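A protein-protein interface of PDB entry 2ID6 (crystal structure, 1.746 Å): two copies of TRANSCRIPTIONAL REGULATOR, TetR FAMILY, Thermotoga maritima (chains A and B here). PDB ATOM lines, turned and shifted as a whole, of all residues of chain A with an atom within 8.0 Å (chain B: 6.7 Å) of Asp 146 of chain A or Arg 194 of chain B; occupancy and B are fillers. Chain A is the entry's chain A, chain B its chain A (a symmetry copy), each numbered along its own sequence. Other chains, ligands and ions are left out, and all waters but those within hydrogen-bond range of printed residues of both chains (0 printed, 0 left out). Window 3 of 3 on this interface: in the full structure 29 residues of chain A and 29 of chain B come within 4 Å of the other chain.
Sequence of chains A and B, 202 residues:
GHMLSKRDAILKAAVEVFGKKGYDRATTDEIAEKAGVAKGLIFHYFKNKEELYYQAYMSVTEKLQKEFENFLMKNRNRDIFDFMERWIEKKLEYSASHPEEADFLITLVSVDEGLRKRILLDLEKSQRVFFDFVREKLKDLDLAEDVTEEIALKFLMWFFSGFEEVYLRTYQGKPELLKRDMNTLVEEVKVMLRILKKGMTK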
ATOM      1  N   LEU A 143      -0.740  15.244  -1.139  1.00  0.00           N
ATOM      2  CA  LEU A 143      -1.750  14.284  -1.581  1.00  0.00           C
ATOM      3  C   LEU A 143      -3.015  14.366  -0.749  1.00  0.00           C
ATOM      4  O   LEU A 143      -2.964  14.716   0.442  1.00  0.00           O
ATOM      5  CB  LEU A 143      -1.200  12.845  -1.614  1.00  0.00           C
ATOM      6  CG  LEU A 143      -0.132  12.469  -2.670  1.00  0.00           C
ATOM      7  CD1 LEU A 143       0.357  11.026  -2.500  1.00  0.00           C
ATOM      8  CD2 LEU A 143      -0.628  12.664  -4.083  1.00  0.00           C
ATOM      9  N   ALA A 144      -4.152  14.036  -1.368  1.00  0.00           N
ATOM     10  CA  ALA A 144      -5.410  13.971  -0.628  1.00  0.00           C
ATOM     11  C   ALA A 144      -5.168  13.013   0.530  1.00  0.00           C
ATOM     12  O   ALA A 144      -4.253  12.181   0.474  1.00  0.00           O
ATOM     13  CB  ALA A 144      -6.545  13.488  -1.519  1.00  0.00           C
ATOM     14  N   GLU A 145      -5.950  13.160   1.596  1.00  0.00           N
ATOM     15  CA  GLU A 145      -5.790  12.306   2.770  1.00  0.00           C
ATOM     16  C   GLU A 145      -6.065  10.834   2.467  1.00  0.00           C
ATOM     17  O   GLU A 145      -5.528   9.954   3.136  1.00  0.00           O
ATOM     18  N   ASP A 146      -6.893  10.559   1.459  1.00  0.00           N
ATOM     19  CA  ASP A 146      -7.221   9.167   1.132  1.00  0.00           C
ATOM     20  C   ASP A 146      -6.369   8.561   0.003  1.00  0.00           C
ATOM     21  O   ASP A 146      -6.555   7.396  -0.382  1.00  0.00           O
ATOM     22  CB  ASP A 146      -8.717   9.036   0.823  1.00  0.00           C
ATOM     23  CG  ASP A 146      -9.165   9.919  -0.340  1.00  0.00           C
ATOM     24  OD1 ASP A 146      -8.361  10.717  -0.861  1.00  0.00           O
ATOM     25  OD2 ASP A 146     -10.359   9.837  -0.718  1.00  0.00           O
ATOM     26  N   VAL A 147      -5.413   9.327  -0.514  1.00  0.00           N
ATOM     27  CA  VAL A 147      -4.632   8.824  -1.658  1.00  0.00           C
ATOM     28  C   VAL A 147      -3.202   8.522  -1.233  1.00  0.00           C
ATOM     29  O   VAL A 147      -2.472   9.421  -0.806  1.00  0.00           O
ATOM     30  CB  VAL A 147      -4.630   9.801  -2.846  1.00  0.00           C
ATOM     31  CG1 VAL A 147      -3.754   9.262  -4.000  1.00  0.00           C
ATOM     32  CG2 VAL A 147      -6.046  10.064  -3.330  1.00  0.00           C
ATOM     33  N   THR A 148      -2.826   7.257  -1.351  1.00  0.00           N
ATOM     34  CA  THR A 148      -1.492   6.812  -0.982  1.00  0.00           C
ATOM     35  C   THR A 148      -0.493   7.151  -2.079  1.00  0.00           C
ATOM     36  O   THR A 148      -0.876   7.285  -3.251  1.00  0.00           O
ATOM     37  CB  THR A 148      -1.442   5.289  -0.735  1.00  0.00           C
ATOM     38  OG1 THR A 148      -1.752   4.588  -1.941  1.00  0.00           O
ATOM     39  CG2 THR A 148      -2.422   4.860   0.371  1.00  0.00           C
ATOM     40  N   GLU A 149       0.779   7.297  -1.698  1.00  0.00           N
ATOM     41  CA  GLU A 149       1.847   7.502  -2.692  1.00  0.00           C
ATOM     42  C   GLU A 149       1.848   6.370  -3.728  1.00  0.00           C
ATOM     43  O   GLU A 149       2.131   6.604  -4.909  1.00  0.00           O
ATOM     44  CB  GLU A 149       3.227   7.656  -2.018  1.00  0.00           C
ATOM     45  CG  GLU A 149       3.536   9.121  -1.610  1.00  0.00           C
ATOM     46  CD  GLU A 149       4.782   9.311  -0.756  1.00  0.00           C
ATOM     47  OE1 GLU A 149       5.887   8.980  -1.230  1.00  0.00           O
ATOM     48  OE2 GLU A 149       4.665   9.825   0.391  1.00  0.00           O
ATOM     49  N   ILE A 151      -0.845   4.367  -4.893  1.00  0.00           N
ATOM     50  CA  ILE A 151      -1.932   4.548  -5.877  1.00  0.00           C
ATOM     51  C   ILE A 151      -1.618   5.725  -6.809  1.00  0.00           C
ATOM     52  O   ILE A 151      -1.836   5.625  -8.024  1.00  0.00           O
ATOM     53  CB  ILE A 151      -3.341   4.662  -5.182  1.00  0.00           C
ATOM     54  CG1 ILE A 151      -3.736   3.295  -4.624  1.00  0.00           C
ATOM     55  CG2 ILE A 151      -4.466   5.130  -6.169  1.00  0.00           C
ATOM     56  N   PHE A 155      -1.292   5.125 -10.802  1.00  0.00           N
ATOM     57  CA  PHE A 155      -2.216   5.824 -11.690  1.00  0.00           C
ATOM     58  C   PHE A 155      -1.431   6.698 -12.663  1.00  0.00           C
ATOM     59  O   PHE A 155      -1.713   6.710 -13.855  1.00  0.00           O
ATOM     60  CB  PHE A 155      -3.190   6.664 -10.853  1.00  0.00           C
ATOM     61  CG  PHE A 155      -4.530   6.931 -11.518  1.00  0.00           C
ATOM     62  CD1 PHE A 155      -4.745   6.663 -12.875  1.00  0.00           C
ATOM     63  CD2 PHE A 155      -5.560   7.507 -10.775  1.00  0.00           C
ATOM     64  CE1 PHE A 155      -6.013   6.957 -13.487  1.00  0.00           C
ATOM     65  CE2 PHE A 155      -6.807   7.781 -11.347  1.00  0.00           C
ATOM     66  CZ  PHE A 155      -7.034   7.514 -12.704  1.00  0.00           C
ATOM     67  N   ILE A 195      -6.883  17.210 -14.405  1.00  0.00           N
ATOM     68  CA  ILE A 195      -7.907  16.438 -13.703  1.00  0.00           C
ATOM     69  C   ILE A 195      -7.219  15.486 -12.703  1.00  0.00           C
ATOM     70  O   ILE A 195      -7.619  15.363 -11.570  1.00  0.00           O
ATOM     71  CB  ILE A 195      -8.745  15.635 -14.716  1.00  0.00           C
ATOM     72  CG1 ILE A 195      -9.719  16.582 -15.456  1.00  0.00           C
ATOM     73  CG2 ILE A 195      -9.480  14.466 -14.057  1.00  0.00           C
ATOM     74  CD1 ILE A 195     -10.328  15.960 -16.752  1.00  0.00           C
ATOM     75  N   LYS A 198      -5.734  17.536  -9.671  1.00  0.00           N
ATOM     76  CA  LYS A 198      -6.814  17.985  -8.785  1.00  0.00           C
ATOM     77  C   LYS A 198      -7.363  16.834  -7.966  1.00  0.00           C
ATOM     78  O   LYS A 198      -7.586  16.986  -6.778  1.00  0.00           O
ATOM     79  CB  LYS A 198      -7.940  18.658  -9.554  1.00  0.00           C
ATOM     80  CG  LYS A 198      -9.114  19.052  -8.614  1.00  0.00           C
ATOM     81  CD  LYS A 198     -10.312  19.584  -9.381  1.00  0.00           C
ATOM     82  CE  LYS A 198     -11.479  19.831  -8.411  1.00  0.00           C
ATOM     83  NZ  LYS A 198     -12.752  20.145  -9.090  1.00  0.00           N
ATOM     84  N   GLY A 199      -7.579  15.673  -8.597  1.00  0.00           N
ATOM     85  CA  GLY A 199      -8.149  14.528  -7.898  1.00  0.00           C
ATOM     86  C   GLY A 199      -7.231  13.855  -6.900  1.00  0.00           C
ATOM     87  O   GLY A 199      -7.699  13.209  -5.963  1.00  0.00           O
ATOM     88  N   MET A 200      -5.929  13.983  -7.120  1.00  0.00           N
ATOM     89  CA  MET A 200      -4.919  13.343  -6.297  1.00  0.00           C
ATOM     90  C   MET A 200      -4.511  14.181  -5.117  1.00  0.00           C
ATOM     91  O   MET A 200      -4.025  13.638  -4.140  1.00  0.00           O
ATOM     92  CB  MET A 200      -3.636  13.066  -7.116  1.00  0.00           C
ATOM     93  CG  MET A 200      -3.806  11.998  -8.041  1.00  0.00           C
ATOM     94  SD  MET A 200      -2.056  11.576  -8.764  1.00  0.00           S
ATOM     95  CE  MET A 200      -2.776  10.273  -9.863  1.00  0.00           C
ATOM     96  N   THR A 201      -4.665  15.488  -5.231  1.00  0.00           N
ATOM     97  CA  THR A 201      -4.073  16.422  -4.263  1.00  0.00           C
ATOM     98  C   THR A 201      -5.114  17.072  -3.374  1.00  0.00           C
ATOM     99  O   THR A 201      -6.287  17.099  -3.707  1.00  0.00           O
ATOM    100  CB  THR A 201      -3.286  17.549  -4.982  1.00  0.00           C
ATOM    101  OG1 THR A 201      -4.152  18.238  -5.890  1.00  0.00           O
ATOM    102  CG2 THR A 201      -2.089  16.989  -5.720  1.00  0.00           C
ATOM    103  N   LYS A 202      -4.677  17.658  -2.254  1.00  0.00           N
ATOM    104  CA  LYS A 202      -5.605  18.384  -1.392  1.00  0.00           C
ATOM    105  C   LYS A 202      -6.156  19.652  -2.045  1.00  0.00           C
ATOM    106  O   LYS A 202      -7.271  20.105  -1.776  1.00  0.00           O
ATOM    107  CB  LYS A 202      -4.950  18.690  -0.048  1.00  0.00           C
ATOM    108  CG  LYS A 202      -4.889  17.468   0.841  1.00  0.00           C
ATOM    109  OXT LYS A 202      -5.520  20.263  -2.898  1.00  0.00           O
ATOM    110  N   PHE B  81     -19.958   6.704 -11.978  1.00  0.00           N
ATOM    111  CA  PHE B  81     -18.736   6.130 -11.377  1.00  0.00           C
ATOM    112  C   PHE B  81     -19.046   4.877 -10.583  1.00  0.00           C
ATOM    113  O   PHE B  81     -18.291   3.919 -10.625  1.00  0.00           O
ATOM    114  CB  PHE B  81     -17.985   7.163 -10.516  1.00  0.00           C
ATOM    115  CG  PHE B  81     -17.492   8.345 -11.310  1.00  0.00           C
ATOM    116  CD1 PHE B  81     -18.310   9.454 -11.488  1.00  0.00           C
ATOM    117  CD2 PHE B  81     -16.225   8.345 -11.874  1.00  0.00           C
ATOM    118  CE1 PHE B  81     -17.886  10.562 -12.244  1.00  0.00           C
ATOM    119  CE2 PHE B  81     -15.788   9.437 -12.628  1.00  0.00           C
ATOM    120  CZ  PHE B  81     -16.625  10.547 -12.815  1.00  0.00           C
ATOM    121  N   GLU B 187     -10.039  -2.463  -4.641  1.00  0.00           N
ATOM    122  CA  GLU B 187      -9.858  -1.299  -3.777  1.00  0.00           C
ATOM    123  C   GLU B 187      -9.140  -0.199  -4.548  1.00  0.00           C
ATOM    124  O   GLU B 187      -9.460   0.989  -4.394  1.00  0.00           O
ATOM    125  CB  GLU B 187      -9.115  -1.652  -2.480  1.00  0.00           C
ATOM    126  CG  GLU B 187      -9.104  -0.520  -1.488  1.00  0.00           C
ATOM    127  CD  GLU B 187     -10.476   0.169  -1.338  1.00  0.00           C
ATOM    128  OE1 GLU B 187     -11.482  -0.525  -1.000  1.00  0.00           O
ATOM    129  OE2 GLU B 187     -10.533   1.411  -1.552  1.00  0.00           O
ATOM    130  N   VAL B 189      -9.158   0.339  -7.900  1.00  0.00           N
ATOM    131  CA  VAL B 189     -10.160   0.871  -8.832  1.00  0.00           C
ATOM    132  C   VAL B 189     -11.068   1.908  -8.169  1.00  0.00           C
ATOM    133  O   VAL B 189     -11.306   2.990  -8.729  1.00  0.00           O
ATOM    134  CB  VAL B 189     -11.022  -0.277  -9.378  1.00  0.00           C
ATOM    135  CG1 VAL B 189     -12.313   0.243 -10.027  1.00  0.00           C
ATOM    136  CG2 VAL B 189     -10.214  -1.057 -10.351  1.00  0.00           C
ATOM    137  N   LYS B 190     -11.572   1.562  -6.987  1.00  0.00           N
ATOM    138  CA  LYS B 190     -12.442   2.492  -6.241  1.00  0.00           C
ATOM    139  C   LYS B 190     -11.741   3.824  -6.036  1.00  0.00           C
ATOM    140  O   LYS B 190     -12.330   4.906  -6.261  1.00  0.00           O
ATOM    141  CB  LYS B 190     -12.876   1.892  -4.906  1.00  0.00           C
ATOM    142  CG  LYS B 190     -13.940   0.800  -5.010  1.00  0.00           C
ATOM    143  CD  LYS B 190     -14.210   0.218  -3.594  1.00  0.00           C
ATOM    144  CE  LYS B 190     -15.153  -1.002  -3.686  1.00  0.00           C
ATOM    145  NZ  LYS B 190     -15.365  -1.645  -2.348  1.00  0.00           N
ATOM    146  N   VAL B 191     -10.480   3.774  -5.600  1.00  0.00           N
ATOM    147  CA  VAL B 191      -9.753   5.027  -5.319  1.00  0.00           C
ATOM    148  C   VAL B 191      -9.464   5.810  -6.618  1.00  0.00           C
ATOM    149  O   VAL B 191      -9.625   7.027  -6.685  1.00  0.00           O
ATOM    150  CB  VAL B 191      -8.459   4.764  -4.559  1.00  0.00           C
ATOM    151  CG1 VAL B 191      -7.705   6.112  -4.281  1.00  0.00           C
ATOM    152  CG2 VAL B 191      -8.769   3.981  -3.263  1.00  0.00           C
ATOM    153  N   MET B 192      -9.046   5.107  -7.662  1.00  0.00           N
ATOM    154  CA  MET B 192      -8.803   5.772  -8.932  1.00  0.00           C
ATOM    155  C   MET B 192     -10.070   6.429  -9.485  1.00  0.00           C
ATOM    156  O   MET B 192     -10.014   7.552  -9.989  1.00  0.00           O
ATOM    157  CB  MET B 192      -8.180   4.776  -9.925  1.00  0.00           C
ATOM    158  CG  MET B 192      -6.870   4.355  -9.364  1.00  0.00           C
ATOM    159  SD  MET B 192      -5.841   3.318 -10.688  1.00  0.00           S
ATOM    160  CE  MET B 192      -4.517   2.673  -9.432  1.00  0.00           C
ATOM    161  N   LEU B 193     -11.207   5.751  -9.358  1.00  0.00           N
ATOM    162  CA  LEU B 193     -12.440   6.322  -9.867  1.00  0.00           C
ATOM    163  C   LEU B 193     -12.816   7.535  -9.040  1.00  0.00           C
ATOM    164  O   LEU B 193     -13.340   8.511  -9.583  1.00  0.00           O
ATOM    165  CB  LEU B 193     -13.589   5.297  -9.921  1.00  0.00           C
ATOM    166  CG  LEU B 193     -13.523   4.379 -11.159  1.00  0.00           C
ATOM    167  CD1 LEU B 193     -14.469   3.219 -11.017  1.00  0.00           C
ATOM    168  CD2 LEU B 193     -13.820   5.142 -12.421  1.00  0.00           C
ATOM    169  N   ARG B 194     -12.558   7.469  -7.738  1.00  0.00           N
ATOM    170  CA  ARG B 194     -12.799   8.637  -6.868  1.00  0.00           C
ATOM    171  C   ARG B 194     -11.902   9.810  -7.271  1.00  0.00           C
ATOM    172  O   ARG B 194     -12.332  10.946  -7.262  1.00  0.00           O
ATOM    173  CB  ARG B 194     -12.621   8.259  -5.392  1.00  0.00           C
ATOM    174  CG  ARG B 194     -13.826   7.516  -4.793  1.00  0.00           C
ATOM    175  CD  ARG B 194     -13.754   7.422  -3.250  1.00  0.00           C
ATOM    176  NE  ARG B 194     -13.330   6.087  -2.806  1.00  0.00           N
ATOM    177  CZ  ARG B 194     -12.330   5.844  -1.959  1.00  0.00           C
ATOM    178  NH1 ARG B 194     -11.625   6.840  -1.421  1.00  0.00           N
ATOM    179  NH2 ARG B 194     -12.028   4.585  -1.649  1.00  0.00           N
ATOM    180  N   ILE B 195     -10.640   9.529  -7.601  1.00  0.00           N
ATOM    181  CA  ILE B 195      -9.729  10.580  -8.049  1.00  0.00           C
ATOM    182  C   ILE B 195     -10.285  11.206  -9.345  1.00  0.00           C
ATOM    183  O   ILE B 195     -10.319  12.403  -9.505  1.00  0.00           O
ATOM    184  CB  ILE B 195      -8.329   9.990  -8.299  1.00  0.00           C
ATOM    185  CG1 ILE B 195      -7.627   9.718  -6.948  1.00  0.00           C
ATOM    186  CG2 ILE B 195      -7.482  10.881  -9.210  1.00  0.00           C
ATOM    187  CD1 ILE B 195      -6.387   8.776  -7.068  1.00  0.00           C
ATOM    188  N   LEU B 196     -10.695  10.375 -10.299  1.00  0.00           N
ATOM    189  CA  LEU B 196     -11.282  10.935 -11.525  1.00  0.00           C
ATOM    190  C   LEU B 196     -12.514  11.784 -11.299  1.00  0.00           C
ATOM    191  O   LEU B 196     -12.623  12.869 -11.865  1.00  0.00           O
ATOM    192  CB  LEU B 196     -11.620   9.823 -12.515  1.00  0.00           C
ATOM    193  CG  LEU B 196     -10.440   9.173 -13.171  1.00  0.00           C
ATOM    194  CD1 LEU B 196     -11.048   8.102 -14.053  1.00  0.00           C
ATOM    195  CD2 LEU B 196      -9.648  10.176 -14.026  1.00  0.00           C
ATOM    196  N   LYS B 197     -13.447  11.288 -10.482  1.00  0.00           N
ATOM    197  CA  LYS B 197     -14.665  12.040 -10.172  1.00  0.00           C
ATOM    198  C   LYS B 197     -14.335  13.394  -9.547  1.00  0.00           C
ATOM    199  O   LYS B 197     -14.874  14.429  -9.968  1.00  0.00           O
ATOM    200  CB  LYS B 197     -15.561  11.238  -9.217  1.00  0.00           C
ATOM    201  CG  LYS B 197     -16.867  11.971  -8.860  1.00  0.00           C
ATOM    202  CD  LYS B 197     -18.006  11.063  -8.412  1.00  0.00           C
ATOM    203  CE  LYS B 197     -19.340  11.890  -8.468  1.00  0.00           C
ATOM    204  NZ  LYS B 197     -20.641  11.099  -8.332  1.00  0.00           N
ATOM    205  N   LYS B 198     -13.478  13.389  -8.543  1.00  0.00           N
ATOM    206  CA  LYS B 198     -13.085  14.641  -7.887  1.00  0.00           C
ATOM    207  C   LYS B 198     -12.460  15.603  -8.877  1.00  0.00           C
ATOM    208  O   LYS B 198     -12.772  16.781  -8.861  1.00  0.00           O
ATOM    209  CB  LYS B 198     -12.134  14.402  -6.724  1.00  0.00           C
ATOM    210  CG  LYS B 198     -11.659  15.742  -6.094  1.00  0.00           C
ATOM    211  CD  LYS B 198     -10.591  15.533  -5.034  1.00  0.00           C
ATOM    212  CE  LYS B 198     -10.074  16.896  -4.545  1.00  0.00           C
ATOM    213  NZ  LYS B 198      -8.888  16.796  -3.673  1.00  0.00           N
ATOM    214  N   GLY B 199     -11.574  15.106  -9.749  1.00  0.00           N
ATOM    215  CA  GLY B 199     -10.890  15.966 -10.705  1.00  0.00           C
ATOM    216  C   GLY B 199     -11.751  16.499 -11.830  1.00  0.00           C
ATOM    217  O   GLY B 199     -11.442  17.540 -12.410  1.00  0.00           O
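Ile 195 of chain A touches Gly 199 of chain B, and with the chains exchanged Gly 199 of chain A touches Ile 195 of chain B. Lys 198 of chain A touches its own counterpart, Lys 198 of chain B. Lys 198 of chain A touches Gly 199 of chain B, and with the chains exchanged Gly 199 of chain A touches Lys 198 of chain B. Gly 199 of chain A touches its own counterpart, Gly 199 of chain B. Positions printed for both chains: 195, 198 and 199.
Among the printed residues, pairs that only touch across the chains: Gly 199 of chain A with Ile 195 of chain B (3.4 Å), Ile 195 of chain A with Gly 199 of chain B (3.4 Å), Phe 155 of chain A with Met 192 of chain B (3.5 Å), Phe 155 of chain A with Leu 196 of chain B (3.8 Å), Gly 199 of chain A with Lys 198 of chain B (3.8 Å), Lys 198 of chain A with Gly 199 of chain B (3.8 Å), Phe 155 of chain A with Ile 195 of chain B (3.8 Å), Ile 151 of chain A with Val 191 of chain B (3.9 Å), Gly 199 of chain A with Gly 199 of chain B (3.9 Å) and Val 147 of chain A with Ile 195 of chain B (3.96 Å).
Of chain B, only Arg 194 (3.3 Å) comes within 4 Å of Asp 146 of chain A. Of the printed residues of chain A, Arg 194 of chain B touches Asp 146 (3.3 Å). Printed residues of chain A within 4 Å of Gly 199 of chain B: Ile 195 (3.4 Å), Lys 198 (3.8 Å) and Gly 199 (3.9 Å). Of the printed residues of chain A, Ile 195 of chain B touches Val 147 (3.96 Å), Phe 155 (3.8 Å) and Gly 199 (3.4 Å). Of the printed residues of chain B, Ile 151 of chain A touches Val 191 (3.9 Å). Of the printed residues of chain B, Val 147 of chain A touches Ile 195. Of the printed residues of chain B, Phe 155 of chain A touches Met 192, Ile 195 and Leu 196. The nearest residue of chain B that does not touch Asp 146 of chain A is Val 191 of chain B (4.3 Å).
Of the 13 printed residues of chain B, 7 touch a printed residue of chain A. Hydrophobic or aromatic side chains of chain A that line the printed part of chain B: Val 147, Ile 151, Phe 155 and Ile 195.
NZ of Lys 198 of chain B lies within hydrogen-bond range of O of Thr 201 of chain A, 2.6 Å away. OD2 of Asp 146 of chain A lies within salt-bridge range of NH1 of Arg 194 of chain B, at 3.3 Å. The backbone carbonyl oxygen (O) of Lys 198 of chain A sits close to the side-chain amino group (NZ) of Lys 198 of chain B, at 3.4 Å.
The guanidinium group (NH2) of Arg 194 of chain B is in salt-bridge range of the side-chain carboxylate (OE2) of Glu 187 of chain B (3.5 Å). OG1 of Thr 148 of chain A lies within hydrogen-bond range of N of Ile 151 of chain A, at 3.1 Å.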
